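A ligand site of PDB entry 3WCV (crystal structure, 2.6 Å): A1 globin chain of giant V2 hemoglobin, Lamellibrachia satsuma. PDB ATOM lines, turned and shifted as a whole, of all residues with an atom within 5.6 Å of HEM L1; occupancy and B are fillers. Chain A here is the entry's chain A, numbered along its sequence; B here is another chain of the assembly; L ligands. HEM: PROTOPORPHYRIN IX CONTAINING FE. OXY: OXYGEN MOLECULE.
ND1 of His 94 of chain A is in hydrogen-bond range of O of Leu 90 (2.7 Å). O of Gln 93 lies within hydrogen-bond range of NH1 of Arg 97 (3.3 Å). The backbone carbonyl oxygen (O) of Phe 104 sits at hydrogen-bond distance from the side-chain hydroxyl (OH) of Tyr 132, at 2.6 Å.
FE of HEM L1 is bound by NE2 of His 94 of chain A, 2.1 Å away. The side-chain hydroxyl (OG) of Ser 48 sits at hydrogen-bond distance from an oxygen (O1D) of HEM L1 (2.6 Å). The side-chain amide nitrogen (NE2) of Gln 98 of chain B lies within hydrogen-bond range of an oxygen (O2A) of HEM L1 (2.8 Å). A ring nitrogen (NE2) of His 94 of chain B sits at hydrogen-bond distance from an oxygen (O2A) of HEM L1. NE2 of His 62 lies within hydrogen-bond range of O2 of OXY L2. NE2 of Gln 93 is in hydrogen-bond range of O2A of HEM L3 (3.5 Å).
FE of HEM L1 is bound by O1 of OXY L2 (1.9 Å).
Residues that only touch HEM L1: Arg 97 (3.3 Å), Val 49 (3.4 Å), Ile 139 (3.4 Å), Phe 104 (3.4 Å), Phe 46 (3.4 Å), Gln 93 (3.5 Å), Arg 65 (3.6 Å), Phe 107 (3.6 Å), Leu 99 (3.6 Å), His 62 (3.7 Å), Leu 45 (3.7 Å), Ile 135 (3.7 Å), Asn 103 (3.8 Å), Tyr 132 (3.9 Å) and Leu 70 (3.96 Å). Hydrophobic or aromatic side chains that line HEM L1: Leu 45, Phe 46, Val 49, His 62, His 94 of chain A, Leu 99, Phe 104, Phe 107, Tyr 132, Ile 135, Ile 139 and His 94 of chain B. The nearest printed residue that does not touch HEM L1 is Val 66 (4.01 Å).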
ATOM      1  N   TRP A  32     -22.635  13.701  32.498  1.00  0.00           N
ATOM      2  CA  TRP A  32     -22.107  14.380  33.659  1.00  0.00           C
ATOM      3  C   TRP A  32     -21.976  13.522  34.926  1.00  0.00           C
ATOM      4  O   TRP A  32     -21.106  13.785  35.782  1.00  0.00           O
ATOM      5  CB  TRP A  32     -22.907  15.660  33.856  1.00  0.00           C
ATOM      6  CG  TRP A  32     -22.507  16.647  32.821  1.00  0.00           C
ATOM      7  CD1 TRP A  32     -23.145  16.903  31.647  1.00  0.00           C
ATOM      8  CD2 TRP A  32     -21.334  17.480  32.823  1.00  0.00           C
ATOM      9  NE1 TRP A  32     -22.452  17.833  30.913  1.00  0.00           N
ATOM     10  CE2 TRP A  32     -21.335  18.202  31.616  1.00  0.00           C
ATOM     11  CE3 TRP A  32     -20.296  17.673  33.732  1.00  0.00           C
ATOM     12  CZ2 TRP A  32     -20.311  19.123  31.277  1.00  0.00           C
ATOM     13  CZ3 TRP A  32     -19.286  18.568  33.417  1.00  0.00           C
ATOM     14  CH2 TRP A  32     -19.298  19.292  32.201  1.00  0.00           C
ATOM     15  N   ALA A  42     -13.471  17.211  39.900  1.00  0.00           N
ATOM     16  CA  ALA A  42     -13.953  18.120  38.871  1.00  0.00           C
ATOM     17  C   ALA A  42     -15.283  18.771  39.206  1.00  0.00           C
ATOM     18  O   ALA A  42     -15.617  19.805  38.634  1.00  0.00           O
ATOM     19  CB  ALA A  42     -14.066  17.396  37.545  1.00  0.00           C
ATOM     20  N   LEU A  45     -15.488  22.422  40.327  1.00  0.00           N
ATOM     21  CA  LEU A  45     -15.234  23.428  39.302  1.00  0.00           C
ATOM     22  C   LEU A  45     -16.533  24.019  38.779  1.00  0.00           C
ATOM     23  O   LEU A  45     -16.515  25.023  38.059  1.00  0.00           O
ATOM     24  CB  LEU A  45     -14.483  22.816  38.115  1.00  0.00           C
ATOM     25  CG  LEU A  45     -13.135  22.164  38.420  1.00  0.00           C
ATOM     26  CD1 LEU A  45     -12.665  21.357  37.224  1.00  0.00           C
ATOM     27  CD2 LEU A  45     -12.139  23.248  38.765  1.00  0.00           C
ATOM     28  N   PHE A  46     -17.663  23.411  39.143  1.00  0.00           N
ATOM     29  CA  PHE A  46     -18.965  23.856  38.660  1.00  0.00           C
ATOM     30  C   PHE A  46     -19.926  24.445  39.675  1.00  0.00           C
ATOM     31  O   PHE A  46     -21.154  24.317  39.527  1.00  0.00           O
ATOM     32  CB  PHE A  46     -19.625  22.697  37.922  1.00  0.00           C
ATOM     33  CG  PHE A  46     -18.835  22.211  36.747  1.00  0.00           C
ATOM     34  CD1 PHE A  46     -19.040  22.742  35.475  1.00  0.00           C
ATOM     35  CD2 PHE A  46     -17.843  21.233  36.920  1.00  0.00           C
ATOM     36  CE1 PHE A  46     -18.256  22.321  34.391  1.00  0.00           C
ATOM     37  CE2 PHE A  46     -17.057  20.803  35.853  1.00  0.00           C
ATOM     38  CZ  PHE A  46     -17.252  21.336  34.581  1.00  0.00           C
ATOM     39  N   SER A  48     -20.539  27.452  40.040  1.00  0.00           N
ATOM     40  CA  SER A  48     -21.234  28.527  39.351  1.00  0.00           C
ATOM     41  C   SER A  48     -22.545  28.068  38.701  1.00  0.00           C
ATOM     42  O   SER A  48     -23.422  28.882  38.417  1.00  0.00           O
ATOM     43  CB  SER A  48     -20.333  29.145  38.271  1.00  0.00           C
ATOM     44  OG  SER A  48     -19.810  28.152  37.380  1.00  0.00           O
ATOM     45  N   VAL A  49     -22.682  26.775  38.459  1.00  0.00           N
ATOM     46  CA  VAL A  49     -23.897  26.251  37.851  1.00  0.00           C
ATOM     47  C   VAL A  49     -24.600  25.275  38.779  1.00  0.00           C
ATOM     48  O   VAL A  49     -25.404  24.450  38.342  1.00  0.00           O
ATOM     49  CB  VAL A  49     -23.627  25.587  36.475  1.00  0.00           C
ATOM     50  CG1 VAL A  49     -23.487  26.650  35.416  1.00  0.00           C
ATOM     51  CG2 VAL A  49     -22.379  24.725  36.521  1.00  0.00           C
ATOM     52  N   HIS A  62     -26.929  23.900  32.422  1.00  0.00           N
ATOM     53  CA  HIS A  62     -25.537  23.737  32.062  1.00  0.00           C
ATOM     54  C   HIS A  62     -25.385  22.486  31.188  1.00  0.00           C
ATOM     55  O   HIS A  62     -24.753  22.520  30.128  1.00  0.00           O
ATOM     56  CB  HIS A  62     -24.674  23.612  33.312  1.00  0.00           C
ATOM     57  CG  HIS A  62     -23.256  23.317  32.995  1.00  0.00           C
ATOM     58  ND1 HIS A  62     -22.430  24.229  32.378  1.00  0.00           N
ATOM     59  CD2 HIS A  62     -22.523  22.184  33.130  1.00  0.00           C
ATOM     60  CE1 HIS A  62     -21.244  23.678  32.160  1.00  0.00           C
ATOM     61  NE2 HIS A  62     -21.276  22.434  32.615  1.00  0.00           N
ATOM     62  N   ARG A  65     -26.613  23.185  27.821  1.00  0.00           N
ATOM     63  CA  ARG A  65     -25.744  24.017  27.021  1.00  0.00           C
ATOM     64  C   ARG A  65     -24.564  23.223  26.480  1.00  0.00           C
ATOM     65  O   ARG A  65     -24.183  23.367  25.310  1.00  0.00           O
ATOM     66  CB  ARG A  65     -25.242  25.232  27.823  1.00  0.00           C
ATOM     67  CG  ARG A  65     -26.252  26.376  27.848  1.00  0.00           C
ATOM     68  CD  ARG A  65     -25.682  27.648  28.453  1.00  0.00           C
ATOM     69  NE  ARG A  65     -25.307  27.518  29.877  1.00  0.00           N
ATOM     70  CZ  ARG A  65     -26.138  27.681  30.919  1.00  0.00           C
ATOM     71  NH1 ARG A  65     -27.414  27.976  30.730  1.00  0.00           N
ATOM     72  NH2 ARG A  65     -25.678  27.583  32.154  1.00  0.00           N
ATOM     73  N   VAL A  66     -23.993  22.378  27.325  1.00  0.00           N
ATOM     74  CA  VAL A  66     -22.849  21.558  26.956  1.00  0.00           C
ATOM     75  C   VAL A  66     -23.139  20.539  25.860  1.00  0.00           C
ATOM     76  O   VAL A  66     -22.344  20.395  24.946  1.00  0.00           O
ATOM     77  CB  VAL A  66     -22.294  20.818  28.183  1.00  0.00           C
ATOM     78  CG1 VAL A  66     -21.189  19.859  27.763  1.00  0.00           C
ATOM     79  CG2 VAL A  66     -21.780  21.810  29.198  1.00  0.00           C
ATOM     80  N   GLY A  69     -23.691  22.184  22.704  1.00  0.00           N
ATOM     81  CA  GLY A  69     -22.414  22.590  22.138  1.00  0.00           C
ATOM     82  C   GLY A  69     -21.768  21.421  21.423  1.00  0.00           C
ATOM     83  O   GLY A  69     -21.292  21.559  20.291  1.00  0.00           O
ATOM     84  N   LEU A  70     -21.732  20.260  22.067  1.00  0.00           N
ATOM     85  CA  LEU A  70     -21.190  19.071  21.425  1.00  0.00           C
ATOM     86  C   LEU A  70     -21.958  18.879  20.114  1.00  0.00           C
ATOM     87  O   LEU A  70     -21.363  18.665  19.059  1.00  0.00           O
ATOM     88  CB  LEU A  70     -21.385  17.860  22.316  1.00  0.00           C
ATOM     89  CG  LEU A  70     -20.294  17.647  23.364  1.00  0.00           C
ATOM     90  CD1 LEU A  70     -20.742  16.660  24.450  1.00  0.00           C
ATOM     91  CD2 LEU A  70     -19.030  17.162  22.625  1.00  0.00           C
ATOM     92  N   ARG A  72     -23.783  21.028  18.114  1.00  0.00           N
ATOM     93  CA  ARG A  72     -23.537  22.010  17.044  1.00  0.00           C
ATOM     94  C   ARG A  72     -22.116  21.846  16.499  1.00  0.00           C
ATOM     95  O   ARG A  72     -21.870  22.053  15.301  1.00  0.00           O
ATOM     96  CB  ARG A  72     -23.730  23.417  17.562  1.00  0.00           C
ATOM     97  CG  ARG A  72     -22.669  23.845  18.528  1.00  0.00           C
ATOM     98  CD  ARG A  72     -23.026  25.172  19.110  1.00  0.00           C
ATOM     99  NE  ARG A  72     -21.817  25.912  19.432  1.00  0.00           N
ATOM    100  CZ  ARG A  72     -21.672  26.655  20.514  1.00  0.00           C
ATOM    101  NH1 ARG A  72     -22.678  26.762  21.351  1.00  0.00           N
ATOM    102  NH2 ARG A  72     -20.535  27.261  20.745  1.00  0.00           N
ATOM    103  N   LEU A  90     -15.776  28.669  21.652  1.00  0.00           N
ATOM    104  CA  LEU A  90     -15.842  27.872  22.877  1.00  0.00           C
ATOM    105  C   LEU A  90     -14.561  28.037  23.668  1.00  0.00           C
ATOM    106  O   LEU A  90     -14.551  27.953  24.921  1.00  0.00           O
ATOM    107  CB  LEU A  90     -16.044  26.399  22.545  1.00  0.00           C
ATOM    108  CG  LEU A  90     -17.324  26.033  21.834  1.00  0.00           C
ATOM    109  CD1 LEU A  90     -17.340  24.549  21.512  1.00  0.00           C
ATOM    110  CD2 LEU A  90     -18.478  26.408  22.726  1.00  0.00           C
ATOM    111  N   GLN A  93     -14.301  31.026  25.775  1.00  0.00           N
ATOM    112  CA  GLN A  93     -15.173  30.893  26.936  1.00  0.00           C
ATOM    113  C   GLN A  93     -14.588  29.993  28.021  1.00  0.00           C
ATOM    114  O   GLN A  93     -14.956  30.115  29.187  1.00  0.00           O
ATOM    115  CB  GLN A  93     -16.543  30.339  26.539  1.00  0.00           C
ATOM    116  CG  GLN A  93     -17.353  31.242  25.624  1.00  0.00           C
ATOM    117  CD  GLN A  93     -18.607  30.582  25.135  1.00  0.00           C
ATOM    118  OE1 GLN A  93     -18.566  29.526  24.511  1.00  0.00           O
ATOM    119  NE2 GLN A  93     -19.743  31.210  25.395  1.00  0.00           N
ATOM    120  N   HIS A  94     -13.709  29.066  27.651  1.00  0.00           N
ATOM    121  CA  HIS A  94     -13.125  28.198  28.652  1.00  0.00           C
ATOM    122  C   HIS A  94     -11.755  28.670  29.142  1.00  0.00           C
ATOM    123  O   HIS A  94     -11.339  28.329  30.262  1.00  0.00           O
ATOM    124  CB  HIS A  94     -13.009  26.763  28.120  1.00  0.00           C
ATOM    125  CG  HIS A  94     -14.321  26.037  28.002  1.00  0.00           C
ATOM    126  ND1 HIS A  94     -15.175  26.231  26.931  1.00  0.00           N
ATOM    127  CD2 HIS A  94     -14.909  25.107  28.788  1.00  0.00           C
ATOM    128  CE1 HIS A  94     -16.225  25.444  27.069  1.00  0.00           C
ATOM    129  NE2 HIS A  94     -16.094  24.757  28.184  1.00  0.00           N
ATOM    130  N   ARG A  97     -11.068  30.426  32.577  1.00  0.00           N
ATOM    131  CA  ARG A  97     -11.401  29.627  33.751  1.00  0.00           C
ATOM    132  C   ARG A  97     -10.226  28.818  34.263  1.00  0.00           C
ATOM    133  O   ARG A  97     -10.385  28.053  35.225  1.00  0.00           O
ATOM    134  CB  ARG A  97     -12.562  28.682  33.444  1.00  0.00           C
ATOM    135  CG  ARG A  97     -13.888  29.400  33.214  1.00  0.00           C
ATOM    136  CD  ARG A  97     -14.805  29.246  34.404  1.00  0.00           C
ATOM    137  NE  ARG A  97     -15.986  30.111  34.305  1.00  0.00           N
ATOM    138  CZ  ARG A  97     -16.750  30.257  33.219  1.00  0.00           C
ATOM    139  NH1 ARG A  97     -16.464  29.588  32.097  1.00  0.00           N
ATOM    140  NH2 ARG A  97     -17.800  31.063  33.250  1.00  0.00           N
ATOM    141  N   LEU A  99      -8.743  26.149  33.304  1.00  0.00           N
ATOM    142  CA  LEU A  99      -9.079  24.728  33.423  1.00  0.00           C
ATOM    143  C   LEU A  99      -7.922  23.787  33.071  1.00  0.00           C
ATOM    144  O   LEU A  99      -7.308  23.917  32.017  1.00  0.00           O
ATOM    145  CB  LEU A  99     -10.278  24.411  32.533  1.00  0.00           C
ATOM    146  CG  LEU A  99     -11.556  25.246  32.749  1.00  0.00           C
ATOM    147  CD1 LEU A  99     -12.608  24.807  31.719  1.00  0.00           C
ATOM    148  CD2 LEU A  99     -12.084  25.045  34.161  1.00  0.00           C
ATOM    149  N   ASN A 103      -8.756  17.370  32.418  1.00  0.00           N
ATOM    150  CA  ASN A 103     -10.181  17.152  32.604  1.00  0.00           C
ATOM    151  C   ASN A 103     -10.904  16.923  31.268  1.00  0.00           C
ATOM    152  O   ASN A 103     -11.929  16.220  31.231  1.00  0.00           O
ATOM    153  CB  ASN A 103     -10.792  18.317  33.380  1.00  0.00           C
ATOM    154  CG  ASN A 103     -10.611  18.160  34.887  1.00  0.00           C
ATOM    155  OD1 ASN A 103     -10.814  19.090  35.642  1.00  0.00           O
ATOM    156  ND2 ASN A 103     -10.254  16.955  35.314  1.00  0.00           N
ATOM    157  N   PHE A 104     -10.371  17.497  30.188  1.00  0.00           N
ATOM    158  CA  PHE A 104     -10.952  17.279  28.870  1.00  0.00           C
ATOM    159  C   PHE A 104     -10.728  15.840  28.444  1.00  0.00           C
ATOM    160  O   PHE A 104     -11.461  15.329  27.601  1.00  0.00           O
ATOM    161  CB  PHE A 104     -10.387  18.255  27.839  1.00  0.00           C
ATOM    162  CG  PHE A 104     -10.955  19.628  27.945  1.00  0.00           C
ATOM    163  CD1 PHE A 104     -11.995  20.025  27.106  1.00  0.00           C
ATOM    164  CD2 PHE A 104     -10.513  20.498  28.933  1.00  0.00           C
ATOM    165  CE1 PHE A 104     -12.592  21.288  27.240  1.00  0.00           C
ATOM    166  CE2 PHE A 104     -11.094  21.736  29.076  1.00  0.00           C
ATOM    167  CZ  PHE A 104     -12.135  22.138  28.227  1.00  0.00           C
ATOM    168  N   PHE A 107     -13.498  14.115  30.304  1.00  0.00           N
ATOM    169  CA  PHE A 107     -14.735  14.406  29.588  1.00  0.00           C
ATOM    170  C   PHE A 107     -14.899  13.402  28.435  1.00  0.00           C
ATOM    171  O   PHE A 107     -15.886  12.648  28.377  1.00  0.00           O
ATOM    172  CB  PHE A 107     -14.715  15.867  29.085  1.00  0.00           C
ATOM    173  CG  PHE A 107     -16.007  16.333  28.476  1.00  0.00           C
ATOM    174  CD1 PHE A 107     -16.415  15.855  27.227  1.00  0.00           C
ATOM    175  CD2 PHE A 107     -16.831  17.239  29.166  1.00  0.00           C
ATOM    176  CE1 PHE A 107     -17.635  16.279  26.677  1.00  0.00           C
ATOM    177  CE2 PHE A 107     -18.053  17.672  28.620  1.00  0.00           C
ATOM    178  CZ  PHE A 107     -18.460  17.193  27.371  1.00  0.00           C
ATOM    179  N   TYR A 132     -12.806  13.265  18.811  1.00  0.00           N
ATOM    180  CA  TYR A 132     -12.975  14.045  20.015  1.00  0.00           C
ATOM    181  C   TYR A 132     -11.726  14.899  20.174  1.00  0.00           C
ATOM    182  O   TYR A 132     -11.827  16.085  20.533  1.00  0.00           O
ATOM    183  CB  TYR A 132     -13.118  13.170  21.258  1.00  0.00           C
ATOM    184  CG  TYR A 132     -13.150  14.005  22.526  1.00  0.00           C
ATOM    185  CD1 TYR A 132     -12.105  13.940  23.452  1.00  0.00           C
ATOM    186  CD2 TYR A 132     -14.203  14.894  22.769  1.00  0.00           C
ATOM    187  CE1 TYR A 132     -12.100  14.747  24.587  1.00  0.00           C
ATOM    188  CE2 TYR A 132     -14.209  15.704  23.896  1.00  0.00           C
ATOM    189  CZ  TYR A 132     -13.152  15.627  24.803  1.00  0.00           C
ATOM    190  OH  TYR A 132     -13.110  16.450  25.918  1.00  0.00           O
ATOM    191  N   ILE A 135     -11.980  18.132  18.747  1.00  0.00           N
ATOM    192  CA  ILE A 135     -12.792  19.056  19.535  1.00  0.00           C
ATOM    193  C   ILE A 135     -12.032  19.645  20.717  1.00  0.00           C
ATOM    194  O   ILE A 135     -11.919  20.863  20.835  1.00  0.00           O
ATOM    195  CB  ILE A 135     -14.088  18.385  19.994  1.00  0.00           C
ATOM    196  CG1 ILE A 135     -14.965  18.140  18.752  1.00  0.00           C
ATOM    197  CG2 ILE A 135     -14.825  19.302  20.970  1.00  0.00           C
ATOM    198  CD1 ILE A 135     -16.216  17.257  18.975  1.00  0.00           C
ATOM    199  N   ALA A 136     -11.465  18.767  21.558  1.00  0.00           N
ATOM    200  CA  ALA A 136     -10.700  19.156  22.731  1.00  0.00           C
ATOM    201  C   ALA A 136      -9.600  20.155  22.375  1.00  0.00           C
ATOM    202  O   ALA A 136      -9.403  21.158  23.060  1.00  0.00           O
ATOM    203  CB  ALA A 136     -10.096  17.901  23.411  1.00  0.00           C
ATOM    204  N   ILE A 139     -10.766  23.608  21.682  1.00  0.00           N
ATOM    205  CA  ILE A 139     -11.219  24.315  22.859  1.00  0.00           C
ATOM    206  C   ILE A 139     -10.095  24.626  23.848  1.00  0.00           C
ATOM    207  O   ILE A 139     -10.125  25.642  24.529  1.00  0.00           O
ATOM    208  CB  ILE A 139     -12.312  23.512  23.583  1.00  0.00           C
ATOM    209  CG1 ILE A 139     -13.517  23.331  22.648  1.00  0.00           C
ATOM    210  CG2 ILE A 139     -12.713  24.203  24.891  1.00  0.00           C
ATOM    211  CD1 ILE A 139     -14.584  22.364  23.150  1.00  0.00           C
ATOM    212  N   HIS B  94     -30.031  32.732  31.313  1.00  0.00           N
ATOM    213  CA  HIS B  94     -28.643  32.712  30.811  1.00  0.00           C
ATOM    214  C   HIS B  94     -28.535  33.392  29.430  1.00  0.00           C
ATOM    215  O   HIS B  94     -27.686  34.256  29.215  1.00  0.00           O
ATOM    216  CB  HIS B  94     -28.123  31.266  30.698  1.00  0.00           C
ATOM    217  CG  HIS B  94     -26.672  31.165  30.326  1.00  0.00           C
ATOM    218  ND1 HIS B  94     -25.649  31.172  31.257  1.00  0.00           N
ATOM    219  CD2 HIS B  94     -26.070  31.082  29.110  1.00  0.00           C
ATOM    220  CE1 HIS B  94     -24.490  31.081  30.630  1.00  0.00           C
ATOM    221  NE2 HIS B  94     -24.709  31.010  29.331  1.00  0.00           N
ATOM    222  N   GLN B  98     -26.625  36.832  28.050  1.00  0.00           N
ATOM    223  CA  GLN B  98     -25.731  36.904  26.902  1.00  0.00           C
ATOM    224  C   GLN B  98     -26.160  37.982  25.915  1.00  0.00           C
ATOM    225  O   GLN B  98     -25.405  38.340  25.009  1.00  0.00           O
ATOM    226  CB  GLN B  98     -25.664  35.559  26.186  1.00  0.00           C
ATOM    227  CG  GLN B  98     -25.023  34.431  27.003  1.00  0.00           C
ATOM    228  CD  GLN B  98     -24.999  33.091  26.263  1.00  0.00           C
ATOM    229  OE1 GLN B  98     -26.040  32.611  25.797  1.00  0.00           O
ATOM    230  NE2 GLN B  98     -23.815  32.479  26.161  1.00  0.00           N
HETATM  231  CHA HEM L   1     -19.383  26.229  30.027  1.00  0.00           C
HETATM  232  CHB HEM L   1     -19.124  23.411  26.257  1.00  0.00           C
HETATM  233  CHC HEM L   1     -15.770  20.777  28.358  1.00  0.00           C
HETATM  234  CHD HEM L   1     -15.995  23.637  32.144  1.00  0.00           C
HETATM  235  C1A HEM L   1     -19.652  25.716  28.774  1.00  0.00           C
HETATM  236  C2A HEM L   1     -20.626  26.244  27.899  1.00  0.00           C
HETATM  237  C3A HEM L   1     -20.549  25.455  26.817  1.00  0.00           C
HETATM  238  C4A HEM L   1     -19.523  24.423  27.059  1.00  0.00           C
HETATM  239  CMA HEM L   1     -21.373  25.529  25.546  1.00  0.00           C
HETATM  240  CAA HEM L   1     -21.549  27.424  28.121  1.00  0.00           C
HETATM  241  CBA HEM L   1     -21.001  28.717  27.589  1.00  0.00           C
HETATM  242  CGA HEM L   1     -21.929  29.919  27.789  1.00  0.00           C
HETATM  243  O1A HEM L   1     -21.624  30.821  28.611  1.00  0.00           O
HETATM  244  O2A HEM L   1     -22.942  29.955  27.148  1.00  0.00           O
HETATM  245  C1B HEM L   1     -18.164  22.386  26.445  1.00  0.00           C
HETATM  246  C2B HEM L   1     -17.859  21.332  25.478  1.00  0.00           C
HETATM  247  C3B HEM L   1     -16.856  20.563  26.126  1.00  0.00           C
HETATM  248  C4B HEM L   1     -16.671  21.201  27.376  1.00  0.00           C
HETATM  249  CMB HEM L   1     -18.486  21.142  24.158  1.00  0.00           C
HETATM  250  CAB HEM L   1     -16.242  19.396  25.551  1.00  0.00           C
HETATM  251  CBB HEM L   1     -15.249  19.414  24.688  1.00  0.00           C
HETATM  252  C1C HEM L   1     -15.543  21.341  29.587  1.00  0.00           C
HETATM  253  C2C HEM L   1     -14.554  20.761  30.546  1.00  0.00           C
HETATM  254  C3C HEM L   1     -14.581  21.572  31.666  1.00  0.00           C
HETATM  255  C4C HEM L   1     -15.631  22.633  31.294  1.00  0.00           C
HETATM  256  CMC HEM L   1     -13.699  19.496  30.292  1.00  0.00           C
HETATM  257  CAC HEM L   1     -13.866  21.434  32.808  1.00  0.00           C
HETATM  258  CBC HEM L   1     -13.819  20.615  33.802  1.00  0.00           C
HETATM  259  C1D HEM L   1     -16.952  24.627  31.915  1.00  0.00           C
HETATM  260  C2D HEM L   1     -17.309  25.716  32.953  1.00  0.00           C
HETATM  261  C3D HEM L   1     -18.284  26.440  32.312  1.00  0.00           C
HETATM  262  C4D HEM L   1     -18.484  25.796  30.960  1.00  0.00           C
HETATM  263  CMD HEM L   1     -16.693  25.871  34.336  1.00  0.00           C
HETATM  264  CAD HEM L   1     -19.030  27.648  32.837  1.00  0.00           C
HETATM  265  CBD HEM L   1     -20.296  27.287  33.537  1.00  0.00           C
HETATM  266  CGD HEM L   1     -21.004  28.476  33.978  1.00  0.00           C
HETATM  267  O1D HEM L   1     -20.915  28.848  35.188  1.00  0.00           O
HETATM  268  O2D HEM L   1     -21.681  29.116  33.126  1.00  0.00           O
HETATM  269  NA  HEM L   1     -18.983  24.603  28.263  1.00  0.00           N
HETATM  270  NB  HEM L   1     -17.474  22.322  27.549  1.00  0.00           N
HETATM  271  NC  HEM L   1     -16.150  22.447  30.085  1.00  0.00           N
HETATM  272  ND  HEM L   1     -17.671  24.731  30.790  1.00  0.00           N
HETATM  273 FE   HEM L   1     -17.554  23.539  29.162  1.00  0.00          FE
HETATM  274  O1  OXY L   2     -18.805  22.492  30.092  1.00  0.00           O
HETATM  275  O2  OXY L   2     -18.718  22.082  31.295  1.00  0.00           O
HETATM  276  CHA HEM L   3     -25.399  35.969  20.418  1.00  0.00           C
HETATM  277  CHB HEM L   3     -29.234  33.177  20.530  1.00  0.00           C
HETATM  278  CHC HEM L   3     -32.004  36.783  18.870  1.00  0.00           C
HETATM  279  CHD HEM L   3     -28.090  39.620  18.847  1.00  0.00           C
HETATM  280  C1A HEM L   3     -26.198  34.878  20.603  1.00  0.00           C
HETATM  281  C2A HEM L   3     -25.723  33.639  21.040  1.00  0.00           C
HETATM  282  C3A HEM L   3     -26.798  32.840  21.086  1.00  0.00           C
HETATM  283  C4A HEM L   3     -27.970  33.599  20.650  1.00  0.00           C
HETATM  284  CMA HEM L   3     -26.821  31.371  21.518  1.00  0.00           C
HETATM  285  CAA HEM L   3     -24.309  33.257  21.391  1.00  0.00           C
HETATM  286  CBA HEM L   3     -23.965  33.472  22.822  1.00  0.00           C
HETATM  287  CGA HEM L   3     -22.533  33.098  23.162  1.00  0.00           C
HETATM  288  O1A HEM L   3     -21.727  33.992  23.510  1.00  0.00           O
HETATM  289  O2A HEM L   3     -22.227  31.941  23.068  1.00  0.00           O
HETATM  290  C1B HEM L   3     -30.369  33.893  20.078  1.00  0.00           C
HETATM  291  C2B HEM L   3     -31.718  33.315  19.949  1.00  0.00           C
HETATM  292  C3B HEM L   3     -32.525  34.395  19.437  1.00  0.00           C
HETATM  293  C4B HEM L   3     -31.633  35.507  19.327  1.00  0.00           C
HETATM  294  CMB HEM L   3     -32.131  31.932  20.257  1.00  0.00           C
HETATM  295  CAB HEM L   3     -33.956  34.269  19.140  1.00  0.00           C
HETATM  296  CBB HEM L   3     -34.926  34.518  19.998  1.00  0.00           C
HETATM  297  C1C HEM L   3     -31.152  37.879  18.735  1.00  0.00           C
HETATM  298  C2C HEM L   3     -31.633  39.194  18.258  1.00  0.00           C
HETATM  299  C3C HEM L   3     -30.519  40.059  18.228  1.00  0.00           C
HETATM  300  C4C HEM L   3     -29.373  39.186  18.723  1.00  0.00           C
HETATM  301  CMC HEM L   3     -33.079  39.508  17.855  1.00  0.00           C
HETATM  302  CAC HEM L   3     -30.493  41.368  17.863  1.00  0.00           C
HETATM  303  CBC HEM L   3     -30.186  42.083  16.842  1.00  0.00           C
HETATM  304  C1D HEM L   3     -27.001  38.865  19.275  1.00  0.00           C
HETATM  305  C2D HEM L   3     -25.575  39.402  19.372  1.00  0.00           C
HETATM  306  C3D HEM L   3     -24.827  38.340  19.811  1.00  0.00           C
HETATM  307  C4D HEM L   3     -25.762  37.210  19.987  1.00  0.00           C
HETATM  308  CMD HEM L   3     -25.161  40.817  19.024  1.00  0.00           C
HETATM  309  CAD HEM L   3     -23.329  38.310  20.077  1.00  0.00           C
HETATM  310  CBD HEM L   3     -22.561  38.021  18.801  1.00  0.00           C
HETATM  311  CGD HEM L   3     -21.093  37.947  18.948  1.00  0.00           C
HETATM  312  O1D HEM L   3     -20.571  36.943  19.517  1.00  0.00           O
HETATM  313  O2D HEM L   3     -20.388  38.844  18.477  1.00  0.00           O
HETATM  314  NA  HEM L   3     -27.577  34.874  20.347  1.00  0.00           N
HETATM  315  NB  HEM L   3     -30.299  35.179  19.705  1.00  0.00           N
HETATM  316  NC  HEM L   3     -29.791  37.930  19.005  1.00  0.00           N
HETATM  317  ND  HEM L   3     -27.038  37.562  19.645  1.00  0.00           N
HETATM  318 FE   HEM L   3     -28.688  36.401  19.699  1.00  0.00          FE
